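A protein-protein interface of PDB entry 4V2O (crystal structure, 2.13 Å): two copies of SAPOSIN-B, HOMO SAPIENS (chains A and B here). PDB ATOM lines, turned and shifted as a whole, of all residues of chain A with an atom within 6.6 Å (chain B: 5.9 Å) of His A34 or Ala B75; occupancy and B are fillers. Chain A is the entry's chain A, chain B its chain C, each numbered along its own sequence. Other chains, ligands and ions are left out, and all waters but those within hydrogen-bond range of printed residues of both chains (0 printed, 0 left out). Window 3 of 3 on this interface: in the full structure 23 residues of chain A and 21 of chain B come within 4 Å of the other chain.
Of the 11 printed residues of chain A, 4 touch a printed residue of chain B. Hydrophobic or aromatic side chains of chain A that line the printed part of chain B: Leu A31, His A34 and Val A35. Of the 12 printed residues of chain B, 5 touch a printed residue of chain A. Among the printed residues, 9 pairs touch across the chains.
No position is printed for both chains. Of the 9 pairs that touch across the chains among the printed residues, none has its exchanged pair printed and touching as well.
Of chain B, only Ala B75, Leu B76, Val B77 and Gly B78 come within 4 Å of His A34. Ala B75 touches just one residue of chain A: His A34. Of the printed residues of chain A, Phe B79 touches Leu A31. Of the printed residues of chain A, Leu B76 touches His A34 and Glu A38. The nearest printed residue of chain B that does not touch Leu A31 is Cys B80 (6.9 Å).
A ring nitrogen (NE2) of His A34 is in hydrogen-bond range of the side-chain carboxylate (OE2) of Glu A38 (3.0 Å). O of Cys B74 sits at hydrogen-bond distance from N of Phe B79, 2.9 Å away.
A ring nitrogen (NE2) of His A34 sits at hydrogen-bond distance from the backbone carbonyl oxygen of Ala B75, 2.7 Å away. The backbone carbonyl oxygen of Leu B76 is in hydrogen-bond range of a ring nitrogen (NE2) of His A34 (3.3 Å).
CD1 of Leu A31 touches O of Val B77, at 3.6 Å. Gly B78 touches Leu A31. Phe B79 touches Leu A31 (CE1 to CD2, 3.98 Å). His A34 touches Val B77 (CD2 to C, 3.9 Å). His A34 touches Gly B78 (CD2 to CA, 3.3 Å). Val B77 touches Val A35. CG of Glu A38 touches O of Leu B76 (3.3 Å).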
ATOM      1  N   GLN A  29      28.271   1.385 -24.068  1.00  0.00           N
ATOM      2  CA  GLN A  29      28.446   1.028 -22.659  1.00  0.00           C
ATOM      3  C   GLN A  29      27.599  -0.190 -22.274  1.00  0.00           C
ATOM      4  O   GLN A  29      28.131  -1.123 -21.674  1.00  0.00           O
ATOM      5  CB  GLN A  29      28.124   2.238 -21.766  1.00  0.00           C
ATOM      6  CG  GLN A  29      28.221   1.978 -20.277  1.00  0.00           C
ATOM      7  CD  GLN A  29      27.967   3.233 -19.485  1.00  0.00           C
ATOM      8  OE1 GLN A  29      26.855   3.774 -19.462  1.00  0.00           O
ATOM      9  NE2 GLN A  29      28.988   3.710 -18.789  1.00  0.00           N
ATOM     10  N   ALA A  30      26.300  -0.194 -22.643  1.00  0.00           N
ATOM     11  CA  ALA A  30      25.384  -1.296 -22.353  1.00  0.00           C
ATOM     12  C   ALA A  30      25.822  -2.592 -23.044  1.00  0.00           C
ATOM     13  O   ALA A  30      25.775  -3.638 -22.404  1.00  0.00           O
ATOM     14  CB  ALA A  30      23.964  -0.939 -22.751  1.00  0.00           C
ATOM     15  N   LEU A  31      26.287  -2.521 -24.312  1.00  0.00           N
ATOM     16  CA  LEU A  31      26.750  -3.683 -25.073  1.00  0.00           C
ATOM     17  C   LEU A  31      28.034  -4.287 -24.468  1.00  0.00           C
ATOM     18  O   LEU A  31      28.086  -5.500 -24.253  1.00  0.00           O
ATOM     19  CB  LEU A  31      26.948  -3.342 -26.566  1.00  0.00           C
ATOM     20  CG  LEU A  31      27.419  -4.484 -27.502  1.00  0.00           C
ATOM     21  CD1 LEU A  31      26.339  -5.525 -27.698  1.00  0.00           C
ATOM     22  CD2 LEU A  31      27.827  -3.948 -28.861  1.00  0.00           C
ATOM     23  N   VAL A  32      29.054  -3.441 -24.200  1.00  0.00           N
ATOM     24  CA  VAL A  32      30.339  -3.855 -23.620  1.00  0.00           C
ATOM     25  C   VAL A  32      30.124  -4.520 -22.247  1.00  0.00           C
ATOM     26  O   VAL A  32      30.662  -5.605 -22.015  1.00  0.00           O
ATOM     27  CB  VAL A  32      31.395  -2.706 -23.597  1.00  0.00           C
ATOM     28  CG1 VAL A  32      32.676  -3.122 -22.880  1.00  0.00           C
ATOM     29  CG2 VAL A  32      31.718  -2.220 -25.007  1.00  0.00           C
ATOM     30  N   GLU A  33      29.292  -3.906 -21.379  1.00  0.00           N
ATOM     31  CA  GLU A  33      28.964  -4.425 -20.046  1.00  0.00           C
ATOM     32  C   GLU A  33      28.227  -5.754 -20.143  1.00  0.00           C
ATOM     33  O   GLU A  33      28.480  -6.632 -19.329  1.00  0.00           O
ATOM     34  CB  GLU A  33      28.107  -3.435 -19.247  1.00  0.00           C
ATOM     35  CG  GLU A  33      28.782  -2.748 -18.091  1.00  0.00           C
ATOM     36  CD  GLU A  33      28.041  -1.486 -17.707  1.00  0.00           C
ATOM     37  OE1 GLU A  33      26.906  -1.572 -17.183  1.00  0.00           O
ATOM     38  OE2 GLU A  33      28.577  -0.399 -18.013  1.00  0.00           O
ATOM     39  N   HIS A  34      27.335  -5.915 -21.143  1.00  0.00           N
ATOM     40  CA  HIS A  34      26.585  -7.153 -21.368  1.00  0.00           C
ATOM     41  C   HIS A  34      27.498  -8.301 -21.765  1.00  0.00           C
ATOM     42  O   HIS A  34      27.360  -9.390 -21.212  1.00  0.00           O
ATOM     43  CB  HIS A  34      25.463  -6.964 -22.399  1.00  0.00           C
ATOM     44  CG  HIS A  34      24.741  -8.237 -22.704  1.00  0.00           C
ATOM     45  ND1 HIS A  34      23.826  -8.772 -21.822  1.00  0.00           N
ATOM     46  CD2 HIS A  34      24.894  -9.086 -23.742  1.00  0.00           C
ATOM     47  CE1 HIS A  34      23.424  -9.905 -22.367  1.00  0.00           C
ATOM     48  NE2 HIS A  34      24.014 -10.124 -23.535  1.00  0.00           N
ATOM     49  N   VAL A  35      28.419  -8.060 -22.726  1.00  0.00           N
ATOM     50  CA  VAL A  35      29.381  -9.054 -23.217  1.00  0.00           C
ATOM     51  C   VAL A  35      30.308  -9.513 -22.061  1.00  0.00           C
ATOM     52  O   VAL A  35      30.596 -10.705 -21.959  1.00  0.00           O
ATOM     53  CB  VAL A  35      30.129  -8.568 -24.498  1.00  0.00           C
ATOM     54  CG1 VAL A  35      31.252  -9.531 -24.901  1.00  0.00           C
ATOM     55  CG2 VAL A  35      29.148  -8.374 -25.665  1.00  0.00           C
ATOM     56  N   LYS A  36      30.693  -8.576 -21.160  1.00  0.00           N
ATOM     57  CA  LYS A  36      31.505  -8.866 -19.971  1.00  0.00           C
ATOM     58  C   LYS A  36      30.752  -9.818 -19.031  1.00  0.00           C
ATOM     59  O   LYS A  36      31.361 -10.739 -18.497  1.00  0.00           O
ATOM     60  CB  LYS A  36      31.890  -7.581 -19.227  1.00  0.00           C
ATOM     61  CG  LYS A  36      33.025  -6.808 -19.872  1.00  0.00           C
ATOM     62  CD  LYS A  36      33.324  -5.541 -19.109  1.00  0.00           C
ATOM     63  CE  LYS A  36      34.306  -4.666 -19.849  1.00  0.00           C
ATOM     64  NZ  LYS A  36      34.616  -3.427 -19.088  1.00  0.00           N
ATOM     65  N   GLU A  37      29.433  -9.618 -18.872  1.00  0.00           N
ATOM     66  CA  GLU A  37      28.553 -10.474 -18.062  1.00  0.00           C
ATOM     67  C   GLU A  37      28.467 -11.889 -18.655  1.00  0.00           C
ATOM     68  O   GLU A  37      28.463 -12.854 -17.895  1.00  0.00           O
ATOM     69  CB  GLU A  37      27.144  -9.866 -17.940  1.00  0.00           C
ATOM     70  CG  GLU A  37      27.068  -8.674 -16.996  1.00  0.00           C
ATOM     71  CD  GLU A  37      25.814  -7.820 -17.070  1.00  0.00           C
ATOM     72  OE1 GLU A  37      24.788  -8.291 -17.614  1.00  0.00           O
ATOM     73  OE2 GLU A  37      25.861  -6.669 -16.576  1.00  0.00           O
ATOM     74  N   GLU A  38      28.451 -12.007 -20.003  1.00  0.00           N
ATOM     75  CA  GLU A  38      28.411 -13.293 -20.705  1.00  0.00           C
ATOM     76  C   GLU A  38      29.667 -14.153 -20.496  1.00  0.00           C
ATOM     77  O   GLU A  38      29.591 -15.374 -20.654  1.00  0.00           O
ATOM     78  CB  GLU A  38      28.090 -13.125 -22.202  1.00  0.00           C
ATOM     79  CG  GLU A  38      26.723 -12.515 -22.476  1.00  0.00           C
ATOM     80  CD  GLU A  38      25.496 -13.295 -22.043  1.00  0.00           C
ATOM     81  OE1 GLU A  38      25.631 -14.474 -21.652  1.00  0.00           O
ATOM     82  OE2 GLU A  38      24.382 -12.742 -22.159  1.00  0.00           O
ATOM     83  N   CYS A  39      30.805 -13.527 -20.122  1.00  0.00           N
ATOM     84  CA  CYS A  39      32.070 -14.222 -19.826  1.00  0.00           C
ATOM     85  C   CYS A  39      31.902 -15.232 -18.670  1.00  0.00           C
ATOM     86  O   CYS A  39      32.639 -16.218 -18.615  1.00  0.00           O
ATOM     87  CB  CYS A  39      33.186 -13.224 -19.529  1.00  0.00           C
ATOM     88  SG  CYS A  39      33.737 -12.260 -20.968  1.00  0.00           S
ATOM     89  N   PRO B  70      16.813 -17.555 -32.882  1.00  0.00           N
ATOM     90  CA  PRO B  70      17.496 -16.310 -33.284  1.00  0.00           C
ATOM     91  C   PRO B  70      17.510 -15.196 -32.225  1.00  0.00           C
ATOM     92  O   PRO B  70      18.547 -14.573 -32.047  1.00  0.00           O
ATOM     93  CB  PRO B  70      16.748 -15.893 -34.551  1.00  0.00           C
ATOM     94  CG  PRO B  70      16.255 -17.187 -35.120  1.00  0.00           C
ATOM     95  CD  PRO B  70      15.837 -17.980 -33.911  1.00  0.00           C
ATOM     96  N   LYS B  71      16.389 -14.987 -31.495  1.00  0.00           N
ATOM     97  CA  LYS B  71      16.288 -13.974 -30.435  1.00  0.00           C
ATOM     98  C   LYS B  71      17.212 -14.289 -29.258  1.00  0.00           C
ATOM     99  O   LYS B  71      17.732 -13.359 -28.644  1.00  0.00           O
ATOM    100  CB  LYS B  71      14.831 -13.771 -29.970  1.00  0.00           C
ATOM    101  CG  LYS B  71      14.156 -14.991 -29.336  1.00  0.00           C
ATOM    102  CD  LYS B  71      12.685 -14.740 -29.090  1.00  0.00           C
ATOM    103  CE  LYS B  71      12.005 -15.949 -28.512  1.00  0.00           C
ATOM    104  NZ  LYS B  71      10.545 -15.721 -28.344  1.00  0.00           N
ATOM    105  N   GLU B  72      17.413 -15.599 -28.949  1.00  0.00           N
ATOM    106  CA  GLU B  72      18.291 -16.068 -27.869  1.00  0.00           C
ATOM    107  C   GLU B  72      19.742 -15.780 -28.200  1.00  0.00           C
ATOM    108  O   GLU B  72      20.471 -15.305 -27.332  1.00  0.00           O
ATOM    109  CB  GLU B  72      18.097 -17.569 -27.587  1.00  0.00           C
ATOM    110  CG  GLU B  72      16.758 -17.904 -26.957  1.00  0.00           C
ATOM    111  CD  GLU B  72      16.453 -19.383 -26.818  1.00  0.00           C
ATOM    112  OE1 GLU B  72      17.039 -20.201 -27.563  1.00  0.00           O
ATOM    113  OE2 GLU B  72      15.595 -19.722 -25.971  1.00  0.00           O
ATOM    114  N   ILE B  73      20.161 -16.057 -29.454  1.00  0.00           N
ATOM    115  CA  ILE B  73      21.523 -15.788 -29.949  1.00  0.00           C
ATOM    116  C   ILE B  73      21.784 -14.276 -29.898  1.00  0.00           C
ATOM    117  O   ILE B  73      22.850 -13.851 -29.452  1.00  0.00           O
ATOM    118  CB  ILE B  73      21.736 -16.373 -31.382  1.00  0.00           C
ATOM    119  CG1 ILE B  73      21.651 -17.921 -31.355  1.00  0.00           C
ATOM    120  CG2 ILE B  73      23.078 -15.919 -31.991  1.00  0.00           C
ATOM    121  CD1 ILE B  73      21.081 -18.566 -32.579  1.00  0.00           C
ATOM    122  N   CYS B  74      20.794 -13.475 -30.327  1.00  0.00           N
ATOM    123  CA  CYS B  74      20.896 -12.011 -30.336  1.00  0.00           C
ATOM    124  C   CYS B  74      20.917 -11.404 -28.949  1.00  0.00           C
ATOM    125  O   CYS B  74      21.637 -10.436 -28.736  1.00  0.00           O
ATOM    126  CB  CYS B  74      19.820 -11.402 -31.220  1.00  0.00           C
ATOM    127  SG  CYS B  74      20.018 -11.821 -32.962  1.00  0.00           S
ATOM    128  N   ALA B  75      20.185 -12.009 -27.996  1.00  0.00           N
ATOM    129  CA  ALA B  75      20.203 -11.585 -26.591  1.00  0.00           C
ATOM    130  C   ALA B  75      21.555 -11.960 -25.974  1.00  0.00           C
ATOM    131  O   ALA B  75      22.089 -11.200 -25.170  1.00  0.00           O
ATOM    132  CB  ALA B  75      19.068 -12.239 -25.819  1.00  0.00           C
ATOM    133  N   LEU B  76      22.128 -13.112 -26.390  1.00  0.00           N
ATOM    134  CA  LEU B  76      23.433 -13.601 -25.924  1.00  0.00           C
ATOM    135  C   LEU B  76      24.565 -12.656 -26.333  1.00  0.00           C
ATOM    136  O   LEU B  76      25.411 -12.335 -25.502  1.00  0.00           O
ATOM    137  CB  LEU B  76      23.689 -15.046 -26.421  1.00  0.00           C
ATOM    138  CG  LEU B  76      25.078 -15.683 -26.192  1.00  0.00           C
ATOM    139  CD1 LEU B  76      25.354 -15.957 -24.719  1.00  0.00           C
ATOM    140  CD2 LEU B  76      25.222 -16.931 -27.002  1.00  0.00           C
ATOM    141  N   VAL B  77      24.570 -12.201 -27.599  1.00  0.00           N
ATOM    142  CA  VAL B  77      25.596 -11.276 -28.099  1.00  0.00           C
ATOM    143  C   VAL B  77      25.416  -9.842 -27.565  1.00  0.00           C
ATOM    144  O   VAL B  77      26.392  -9.112 -27.454  1.00  0.00           O
ATOM    145  CB  VAL B  77      25.808 -11.343 -29.637  1.00  0.00           C
ATOM    146  CG1 VAL B  77      26.309 -12.721 -30.063  1.00  0.00           C
ATOM    147  CG2 VAL B  77      24.536 -10.977 -30.399  1.00  0.00           C
ATOM    148  N   GLY B  78      24.180  -9.474 -27.218  1.00  0.00           N
ATOM    149  CA  GLY B  78      23.855  -8.154 -26.684  1.00  0.00           C
ATOM    150  C   GLY B  78      23.101  -7.236 -27.623  1.00  0.00           C
ATOM    151  O   GLY B  78      22.874  -6.073 -27.285  1.00  0.00           O
ATOM    152  N   PHE B  79      22.696  -7.743 -28.802  1.00  0.00           N
ATOM    153  CA  PHE B  79      21.947  -6.941 -29.777  1.00  0.00           C
ATOM    154  C   PHE B  79      20.450  -6.886 -29.481  1.00  0.00           C
ATOM    155  O   PHE B  79      19.780  -5.970 -29.954  1.00  0.00           O
ATOM    156  CB  PHE B  79      22.259  -7.352 -31.227  1.00  0.00           C
ATOM    157  CG  PHE B  79      23.704  -7.171 -31.641  1.00  0.00           C
ATOM    158  CD1 PHE B  79      24.418  -6.041 -31.261  1.00  0.00           C
ATOM    159  CD2 PHE B  79      24.335  -8.107 -32.451  1.00  0.00           C
ATOM    160  CE1 PHE B  79      25.751  -5.870 -31.655  1.00  0.00           C
ATOM    161  CE2 PHE B  79      25.666  -7.933 -32.847  1.00  0.00           C
ATOM    162  CZ  PHE B  79      26.362  -6.814 -32.447  1.00  0.00           C
ATOM    163  N   CYS B  80      19.940  -7.835 -28.666  1.00  0.00           N
ATOM    164  CA  CYS B  80      18.541  -7.877 -28.218  1.00  0.00           C
ATOM    165  C   CYS B  80      18.485  -7.802 -26.698  1.00  0.00           C
ATOM    166  O   CYS B  80      19.399  -8.292 -26.035  1.00  0.00           O
ATOM    167  CB  CYS B  80      17.812  -9.112 -28.744  1.00  0.00           C
ATOM    168  SG  CYS B  80      17.349  -9.009 -30.490  1.00  0.00           S
ATOM    169  N   ASP B  81      17.398  -7.196 -26.165  1.00  0.00           N
ATOM    170  CA  ASP B  81      17.055  -6.962 -24.748  1.00  0.00           C
ATOM    171  C   ASP B  81      17.664  -5.673 -24.214  1.00  0.00           C
ATOM    172  O   ASP B  81      16.994  -4.641 -24.203  1.00  0.00           O
ATOM    173  CB  ASP B  81      17.374  -8.159 -23.825  1.00  0.00           C
ATOM    174  CG  ASP B  81      16.541  -9.403 -24.063  1.00  0.00           C
ATOM    175  OD1 ASP B  81      16.466  -9.857 -25.227  1.00  0.00           O
ATOM    176  OD2 ASP B  81      16.022  -9.965 -23.073  1.00  0.00           O
